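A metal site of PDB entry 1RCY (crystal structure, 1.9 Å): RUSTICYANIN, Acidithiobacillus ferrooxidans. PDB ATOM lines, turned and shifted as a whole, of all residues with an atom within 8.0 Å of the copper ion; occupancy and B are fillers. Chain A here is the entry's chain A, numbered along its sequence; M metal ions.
ND1 of His 139 is bound to the copper ion (1.9 Å). The copper ion is bound by ND1 of His 81 (2.0 Å). SG of Cys 134 is bound to the copper ion. The copper ion has three donor atoms within binding distance. Slightly farther from the copper ion lies the side-chain sulfur (SD) of Met 144 (2.9 Å).
The backbone carbonyl oxygen (O) of His 139 lies within hydrogen-bond range of the backbone NH (N) of Met 144 (2.9 Å). The backbone carbonyl oxygen (O) of His 139 is in hydrogen-bond range of the side-chain hydroxyl (OG1) of Thr 142 (3.0 Å). ND1 of His 81 lies close to SD of Met 144 (3.4 Å). The side-chain amide oxygen (OD1) of Asn 76 is in hydrogen-bond range of a ring nitrogen (NE2) of His 81. O of His 81 is in hydrogen-bond range of OG of Ser 108 (2.7 Å). The backbone carbonyl oxygen (O) of Met 144 is in hydrogen-bond range of the backbone NH (N) of Cys 134 (3.4 Å). N of Ile 136 sits close to SG of Cys 134. The backbone NH of Ser 82 lies close to the side-chain sulfur of Cys 134 (3.4 Å).
Within 4 Å of the copper ion: His 81, Cys 134, His 139 and Met 144. The nearest printed residue that does not touch the copper ion is Ile 136 (4.02 Å).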
ATOM      1  N   ALA A  40       0.637   9.501 -11.674  1.00  0.00           N
ATOM      2  CA  ALA A  40       0.979   8.477 -10.701  1.00  0.00           C
ATOM      3  C   ALA A  40       2.118   8.967  -9.814  1.00  0.00           C
ATOM      4  O   ALA A  40       3.223   9.236 -10.302  1.00  0.00           O
ATOM      5  CB  ALA A  40       1.364   7.178 -11.400  1.00  0.00           C
ATOM      6  N   VAL A  41       1.816   9.103  -8.527  1.00  0.00           N
ATOM      7  CA  VAL A  41       2.763   9.557  -7.512  1.00  0.00           C
ATOM      8  C   VAL A  41       3.604  10.791  -7.873  1.00  0.00           C
ATOM      9  O   VAL A  41       4.751  10.677  -8.314  1.00  0.00           O
ATOM     10  CB  VAL A  41       3.721   8.409  -7.036  1.00  0.00           C
ATOM     11  CG1 VAL A  41       4.371   8.773  -5.692  1.00  0.00           C
ATOM     12  CG2 VAL A  41       2.972   7.092  -6.917  1.00  0.00           C
ATOM     13  N   PHE A  47       3.170   7.011  -1.563  1.00  0.00           N
ATOM     14  CA  PHE A  47       3.335   5.921  -2.500  1.00  0.00           C
ATOM     15  C   PHE A  47       2.567   4.724  -1.925  1.00  0.00           C
ATOM     16  O   PHE A  47       2.682   4.433  -0.738  1.00  0.00           O
ATOM     17  CB  PHE A  47       4.817   5.557  -2.650  1.00  0.00           C
ATOM     18  CG  PHE A  47       5.067   4.390  -3.575  1.00  0.00           C
ATOM     19  CD1 PHE A  47       5.260   4.592  -4.929  1.00  0.00           C
ATOM     20  CD2 PHE A  47       5.092   3.092  -3.076  1.00  0.00           C
ATOM     21  CE1 PHE A  47       5.466   3.512  -5.794  1.00  0.00           C
ATOM     22  CE2 PHE A  47       5.297   2.013  -3.927  1.00  0.00           C
ATOM     23  CZ  PHE A  47       5.480   2.222  -5.290  1.00  0.00           C
ATOM     24  N   PRO A  48       1.712   4.090  -2.740  1.00  0.00           N
ATOM     25  CA  PRO A  48       1.423   4.428  -4.141  1.00  0.00           C
ATOM     26  C   PRO A  48       0.055   5.119  -4.223  1.00  0.00           C
ATOM     27  O   PRO A  48      -0.882   4.751  -3.511  1.00  0.00           O
ATOM     28  CB  PRO A  48       1.400   3.054  -4.811  1.00  0.00           C
ATOM     29  CG  PRO A  48       0.715   2.211  -3.782  1.00  0.00           C
ATOM     30  CD  PRO A  48       1.295   2.699  -2.455  1.00  0.00           C
ATOM     31  N   SER A  49      -0.063   6.110  -5.103  1.00  0.00           N
ATOM     32  CA  SER A  49      -1.320   6.829  -5.253  1.00  0.00           C
ATOM     33  C   SER A  49      -1.403   7.581  -6.570  1.00  0.00           C
ATOM     34  O   SER A  49      -0.405   7.735  -7.293  1.00  0.00           O
ATOM     35  CB  SER A  49      -1.520   7.828  -4.096  1.00  0.00           C
ATOM     36  OG  SER A  49      -0.512   8.843  -4.071  1.00  0.00           O
ATOM     37  N   PHE A  50      -2.615   8.032  -6.877  1.00  0.00           N
ATOM     38  CA  PHE A  50      -2.918   8.812  -8.065  1.00  0.00           C
ATOM     39  C   PHE A  50      -3.209  10.250  -7.617  1.00  0.00           C
ATOM     40  O   PHE A  50      -3.807  10.466  -6.545  1.00  0.00           O
ATOM     41  CB  PHE A  50      -4.196   8.301  -8.737  1.00  0.00           C
ATOM     42  CG  PHE A  50      -4.051   6.987  -9.454  1.00  0.00           C
ATOM     43  CD1 PHE A  50      -3.320   6.896 -10.637  1.00  0.00           C
ATOM     44  CD2 PHE A  50      -4.696   5.851  -8.971  1.00  0.00           C
ATOM     45  CE1 PHE A  50      -3.250   5.697 -11.334  1.00  0.00           C
ATOM     46  CE2 PHE A  50      -4.623   4.642  -9.667  1.00  0.00           C
ATOM     47  CZ  PHE A  50      -3.905   4.569 -10.845  1.00  0.00           C
ATOM     48  N   PHE A  72      -3.137  10.490 -18.771  1.00  0.00           N
ATOM     49  CA  PHE A  72      -2.431   9.828 -17.680  1.00  0.00           C
ATOM     50  C   PHE A  72      -0.933  10.010 -17.825  1.00  0.00           C
ATOM     51  O   PHE A  72      -0.366   9.660 -18.871  1.00  0.00           O
ATOM     52  CB  PHE A  72      -2.775   8.346 -17.659  1.00  0.00           C
ATOM     53  CG  PHE A  72      -2.037   7.564 -16.605  1.00  0.00           C
ATOM     54  CD1 PHE A  72      -2.125   7.932 -15.265  1.00  0.00           C
ATOM     55  CD2 PHE A  72      -1.253   6.477 -16.948  1.00  0.00           C
ATOM     56  CE1 PHE A  72      -1.452   7.215 -14.291  1.00  0.00           C
ATOM     57  CE2 PHE A  72      -0.572   5.761 -15.981  1.00  0.00           C
ATOM     58  CZ  PHE A  72      -0.670   6.137 -14.650  1.00  0.00           C
ATOM     59  N   ASN A  74       2.806   9.162 -15.930  1.00  0.00           N
ATOM     60  CA  ASN A  74       3.522   8.424 -14.888  1.00  0.00           C
ATOM     61  C   ASN A  74       4.779   9.200 -14.514  1.00  0.00           C
ATOM     62  O   ASN A  74       5.766   9.161 -15.233  1.00  0.00           O
ATOM     63  CB  ASN A  74       3.932   7.034 -15.349  1.00  0.00           C
ATOM     64  CG  ASN A  74       4.770   6.312 -14.323  1.00  0.00           C
ATOM     65  OD1 ASN A  74       4.674   6.599 -13.126  1.00  0.00           O
ATOM     66  ND2 ASN A  74       5.621   5.393 -14.779  1.00  0.00           N
ATOM     67  N   ASN A  76       6.402   8.732 -11.565  1.00  0.00           N
ATOM     68  CA  ASN A  76       7.095   7.953 -10.541  1.00  0.00           C
ATOM     69  C   ASN A  76       8.248   7.118 -11.103  1.00  0.00           C
ATOM     70  O   ASN A  76       8.046   6.165 -11.838  1.00  0.00           O
ATOM     71  CB  ASN A  76       6.083   7.064  -9.817  1.00  0.00           C
ATOM     72  CG  ASN A  76       6.632   6.458  -8.541  1.00  0.00           C
ATOM     73  OD1 ASN A  76       6.331   5.308  -8.230  1.00  0.00           O
ATOM     74  ND2 ASN A  76       7.407   7.230  -7.779  1.00  0.00           N
ATOM     75  N   PHE A  79       8.803   2.720 -11.560  1.00  0.00           N
ATOM     76  CA  PHE A  79       7.568   1.923 -11.625  1.00  0.00           C
ATOM     77  C   PHE A  79       6.742   2.255 -12.854  1.00  0.00           C
ATOM     78  O   PHE A  79       6.728   3.403 -13.316  1.00  0.00           O
ATOM     79  CB  PHE A  79       6.733   2.148 -10.361  1.00  0.00           C
ATOM     80  CG  PHE A  79       7.471   1.855  -9.098  1.00  0.00           C
ATOM     81  CD1 PHE A  79       8.273   2.827  -8.511  1.00  0.00           C
ATOM     82  CD2 PHE A  79       7.432   0.587  -8.527  1.00  0.00           C
ATOM     83  CE1 PHE A  79       9.016   2.551  -7.384  1.00  0.00           C
ATOM     84  CE2 PHE A  79       8.171   0.301  -7.393  1.00  0.00           C
ATOM     85  CZ  PHE A  79       8.971   1.280  -6.821  1.00  0.00           C
ATOM     86  N   GLY A  80       6.060   1.254 -13.396  1.00  0.00           N
ATOM     87  CA  GLY A  80       5.231   1.476 -14.564  1.00  0.00           C
ATOM     88  C   GLY A  80       3.758   1.344 -14.238  1.00  0.00           C
ATOM     89  O   GLY A  80       3.079   0.444 -14.740  1.00  0.00           O
ATOM     90  N   HIS A  81       3.256   2.240 -13.413  1.00  0.00           N
ATOM     91  CA  HIS A  81       1.844   2.212 -13.001  1.00  0.00           C
ATOM     92  C   HIS A  81       0.885   2.262 -14.194  1.00  0.00           C
ATOM     93  O   HIS A  81       1.256   2.678 -15.290  1.00  0.00           O
ATOM     94  CB  HIS A  81       1.537   3.393 -12.073  1.00  0.00           C
ATOM     95  CG  HIS A  81       2.494   3.558 -10.936  1.00  0.00           C
ATOM     96  ND1 HIS A  81       2.329   2.890  -9.755  1.00  0.00           N
ATOM     97  CD2 HIS A  81       3.543   4.418 -10.815  1.00  0.00           C
ATOM     98  CE1 HIS A  81       3.257   3.346  -8.947  1.00  0.00           C
ATOM     99  NE2 HIS A  81       4.017   4.273  -9.545  1.00  0.00           N
ATOM    100  N   SER A  82      -0.362   1.853 -13.971  1.00  0.00           N
ATOM    101  CA  SER A  82      -1.389   1.898 -15.018  1.00  0.00           C
ATOM    102  C   SER A  82      -2.581   2.646 -14.457  1.00  0.00           C
ATOM    103  O   SER A  82      -2.655   2.888 -13.247  1.00  0.00           O
ATOM    104  CB  SER A  82      -1.824   0.494 -15.437  1.00  0.00           C
ATOM    105  OG  SER A  82      -2.339  -0.254 -14.345  1.00  0.00           O
ATOM    106  N   PHE A  83      -3.460   3.096 -15.338  1.00  0.00           N
ATOM    107  CA  PHE A  83      -4.677   3.795 -14.944  1.00  0.00           C
ATOM    108  C   PHE A  83      -5.785   3.044 -15.697  1.00  0.00           C
ATOM    109  O   PHE A  83      -6.012   3.268 -16.883  1.00  0.00           O
ATOM    110  CB  PHE A  83      -4.618   5.266 -15.377  1.00  0.00           C
ATOM    111  CG  PHE A  83      -5.748   6.102 -14.864  1.00  0.00           C
ATOM    112  CD1 PHE A  83      -6.938   6.216 -15.585  1.00  0.00           C
ATOM    113  CD2 PHE A  83      -5.629   6.805 -13.674  1.00  0.00           C
ATOM    114  CE1 PHE A  83      -7.982   7.021 -15.121  1.00  0.00           C
ATOM    115  CE2 PHE A  83      -6.658   7.605 -13.209  1.00  0.00           C
ATOM    116  CZ  PHE A  83      -7.837   7.712 -13.936  1.00  0.00           C
ATOM    117  N   PHE A 107       0.078  -0.971 -18.530  1.00  0.00           N
ATOM    118  CA  PHE A 107       1.312  -0.531 -17.889  1.00  0.00           C
ATOM    119  C   PHE A 107       2.066   0.541 -18.681  1.00  0.00           C
ATOM    120  O   PHE A 107       2.256   0.421 -19.890  1.00  0.00           O
ATOM    121  CB  PHE A 107       2.212  -1.717 -17.583  1.00  0.00           C
ATOM    122  CG  PHE A 107       1.604  -2.701 -16.622  1.00  0.00           C
ATOM    123  CD1 PHE A 107       1.220  -2.308 -15.350  1.00  0.00           C
ATOM    124  CD2 PHE A 107       1.397  -4.028 -17.008  1.00  0.00           C
ATOM    125  CE1 PHE A 107       0.632  -3.210 -14.468  1.00  0.00           C
ATOM    126  CE2 PHE A 107       0.806  -4.942 -16.131  1.00  0.00           C
ATOM    127  CZ  PHE A 107       0.421  -4.528 -14.855  1.00  0.00           C
ATOM    128  N   SER A 108       2.483   1.591 -17.979  1.00  0.00           N
ATOM    129  CA  SER A 108       3.210   2.709 -18.570  1.00  0.00           C
ATOM    130  C   SER A 108       4.722   2.494 -18.526  1.00  0.00           C
ATOM    131  O   SER A 108       5.215   1.662 -17.764  1.00  0.00           O
ATOM    132  CB  SER A 108       2.891   3.985 -17.794  1.00  0.00           C
ATOM    133  OG  SER A 108       3.344   3.904 -16.460  1.00  0.00           O
ATOM    134  N   VAL A 133      -7.931   2.144 -11.076  1.00  0.00           N
ATOM    135  CA  VAL A 133      -6.943   1.433 -10.285  1.00  0.00           C
ATOM    136  C   VAL A 133      -5.648   1.160 -11.058  1.00  0.00           C
ATOM    137  O   VAL A 133      -5.613   1.220 -12.286  1.00  0.00           O
ATOM    138  CB  VAL A 133      -7.486   0.054  -9.822  1.00  0.00           C
ATOM    139  CG1 VAL A 133      -8.912   0.174  -9.276  1.00  0.00           C
ATOM    140  CG2 VAL A 133      -7.451  -0.943 -10.961  1.00  0.00           C
ATOM    141  N   CYS A 134      -4.588   0.848 -10.310  1.00  0.00           N
ATOM    142  CA  CYS A 134      -3.325   0.499 -10.913  1.00  0.00           C
ATOM    143  C   CYS A 134      -3.220  -1.019 -10.802  1.00  0.00           C
ATOM    144  O   CYS A 134      -3.490  -1.585  -9.736  1.00  0.00           O
ATOM    145  CB  CYS A 134      -2.151   1.143 -10.175  1.00  0.00           C
ATOM    146  SG  CYS A 134      -0.551   0.539 -10.807  1.00  0.00           S
ATOM    147  N   GLN A 135      -2.829  -1.673 -11.891  1.00  0.00           N
ATOM    148  CA  GLN A 135      -2.712  -3.129 -11.913  1.00  0.00           C
ATOM    149  C   GLN A 135      -1.394  -3.736 -11.428  1.00  0.00           C
ATOM    150  O   GLN A 135      -1.281  -4.960 -11.359  1.00  0.00           O
ATOM    151  CB  GLN A 135      -3.037  -3.689 -13.298  1.00  0.00           C
ATOM    152  CG  GLN A 135      -4.490  -3.538 -13.702  1.00  0.00           C
ATOM    153  CD  GLN A 135      -4.879  -4.490 -14.817  1.00  0.00           C
ATOM    154  OE1 GLN A 135      -4.933  -4.113 -15.981  1.00  0.00           O
ATOM    155  NE2 GLN A 135      -5.143  -5.739 -14.460  1.00  0.00           N
ATOM    156  N   ILE A 136      -0.397  -2.913 -11.107  1.00  0.00           N
ATOM    157  CA  ILE A 136       0.855  -3.478 -10.623  1.00  0.00           C
ATOM    158  C   ILE A 136       0.533  -4.194  -9.325  1.00  0.00           C
ATOM    159  O   ILE A 136      -0.070  -3.608  -8.425  1.00  0.00           O
ATOM    160  CB  ILE A 136       1.930  -2.407 -10.387  1.00  0.00           C
ATOM    161  CG1 ILE A 136       2.319  -1.779 -11.723  1.00  0.00           C
ATOM    162  CG2 ILE A 136       3.160  -3.009  -9.701  1.00  0.00           C
ATOM    163  CD1 ILE A 136       3.459  -0.787 -11.625  1.00  0.00           C
ATOM    164  N   PRO A 137       0.864  -5.493  -9.237  1.00  0.00           N
ATOM    165  CA  PRO A 137       0.595  -6.298  -8.034  1.00  0.00           C
ATOM    166  C   PRO A 137       0.917  -5.588  -6.720  1.00  0.00           C
ATOM    167  O   PRO A 137       2.015  -5.065  -6.536  1.00  0.00           O
ATOM    168  CB  PRO A 137       1.475  -7.529  -8.251  1.00  0.00           C
ATOM    169  CG  PRO A 137       1.429  -7.704  -9.730  1.00  0.00           C
ATOM    170  CD  PRO A 137       1.595  -6.282 -10.238  1.00  0.00           C
ATOM    171  N   GLY A 138      -0.094  -5.508  -5.856  1.00  0.00           N
ATOM    172  CA  GLY A 138       0.060  -4.876  -4.559  1.00  0.00           C
ATOM    173  C   GLY A 138      -0.341  -3.418  -4.452  1.00  0.00           C
ATOM    174  O   GLY A 138      -0.733  -2.966  -3.379  1.00  0.00           O
ATOM    175  N   HIS A 139      -0.279  -2.669  -5.561  1.00  0.00           N
ATOM    176  CA  HIS A 139      -0.624  -1.245  -5.534  1.00  0.00           C
ATOM    177  C   HIS A 139      -2.057  -0.933  -5.142  1.00  0.00           C
ATOM    178  O   HIS A 139      -2.297  -0.115  -4.253  1.00  0.00           O
ATOM    179  CB  HIS A 139      -0.247  -0.578  -6.861  1.00  0.00           C
ATOM    180  CG  HIS A 139       1.229  -0.464  -7.071  1.00  0.00           C
ATOM    181  ND1 HIS A 139       1.761   0.299  -8.086  1.00  0.00           N
ATOM    182  CD2 HIS A 139       2.242  -1.040  -6.371  1.00  0.00           C
ATOM    183  CE1 HIS A 139       3.068   0.184  -7.970  1.00  0.00           C
ATOM    184  NE2 HIS A 139       3.413  -0.623  -6.948  1.00  0.00           N
ATOM    185  N   ALA A 140      -3.020  -1.565  -5.821  1.00  0.00           N
ATOM    186  CA  ALA A 140      -4.430  -1.341  -5.526  1.00  0.00           C
ATOM    187  C   ALA A 140      -4.700  -1.747  -4.078  1.00  0.00           C
ATOM    188  O   ALA A 140      -5.407  -1.035  -3.345  1.00  0.00           O
ATOM    189  CB  ALA A 140      -5.292  -2.151  -6.474  1.00  0.00           C
ATOM    190  N   THR A 142      -2.742  -1.587  -1.649  1.00  0.00           N
ATOM    191  CA  THR A 142      -2.173  -0.629  -0.710  1.00  0.00           C
ATOM    192  C   THR A 142      -2.739   0.778  -0.857  1.00  0.00           C
ATOM    193  O   THR A 142      -2.180   1.748  -0.332  1.00  0.00           O
ATOM    194  CB  THR A 142      -0.633  -0.583  -0.769  1.00  0.00           C
ATOM    195  OG1 THR A 142      -0.200  -0.706  -2.136  1.00  0.00           O
ATOM    196  CG2 THR A 142      -0.037  -1.713   0.049  1.00  0.00           C
ATOM    197  N   MET A 144      -3.806   2.346  -4.083  1.00  0.00           N
ATOM    198  CA  MET A 144      -3.713   3.055  -5.344  1.00  0.00           C
ATOM    199  C   MET A 144      -4.956   2.860  -6.215  1.00  0.00           C
ATOM    200  O   MET A 144      -4.963   2.073  -7.163  1.00  0.00           O
ATOM    201  CB  MET A 144      -2.445   2.679  -6.108  1.00  0.00           C
ATOM    202  CG  MET A 144      -2.107   3.654  -7.217  1.00  0.00           C
ATOM    203  SD  MET A 144      -0.464   3.449  -7.908  1.00  0.00           S
ATOM    204  CE  MET A 144      -0.423   4.812  -9.035  1.00  0.00           C
HETATM  205 CU    CU M   1       0.961   1.425  -9.377  1.00  0.00          CU
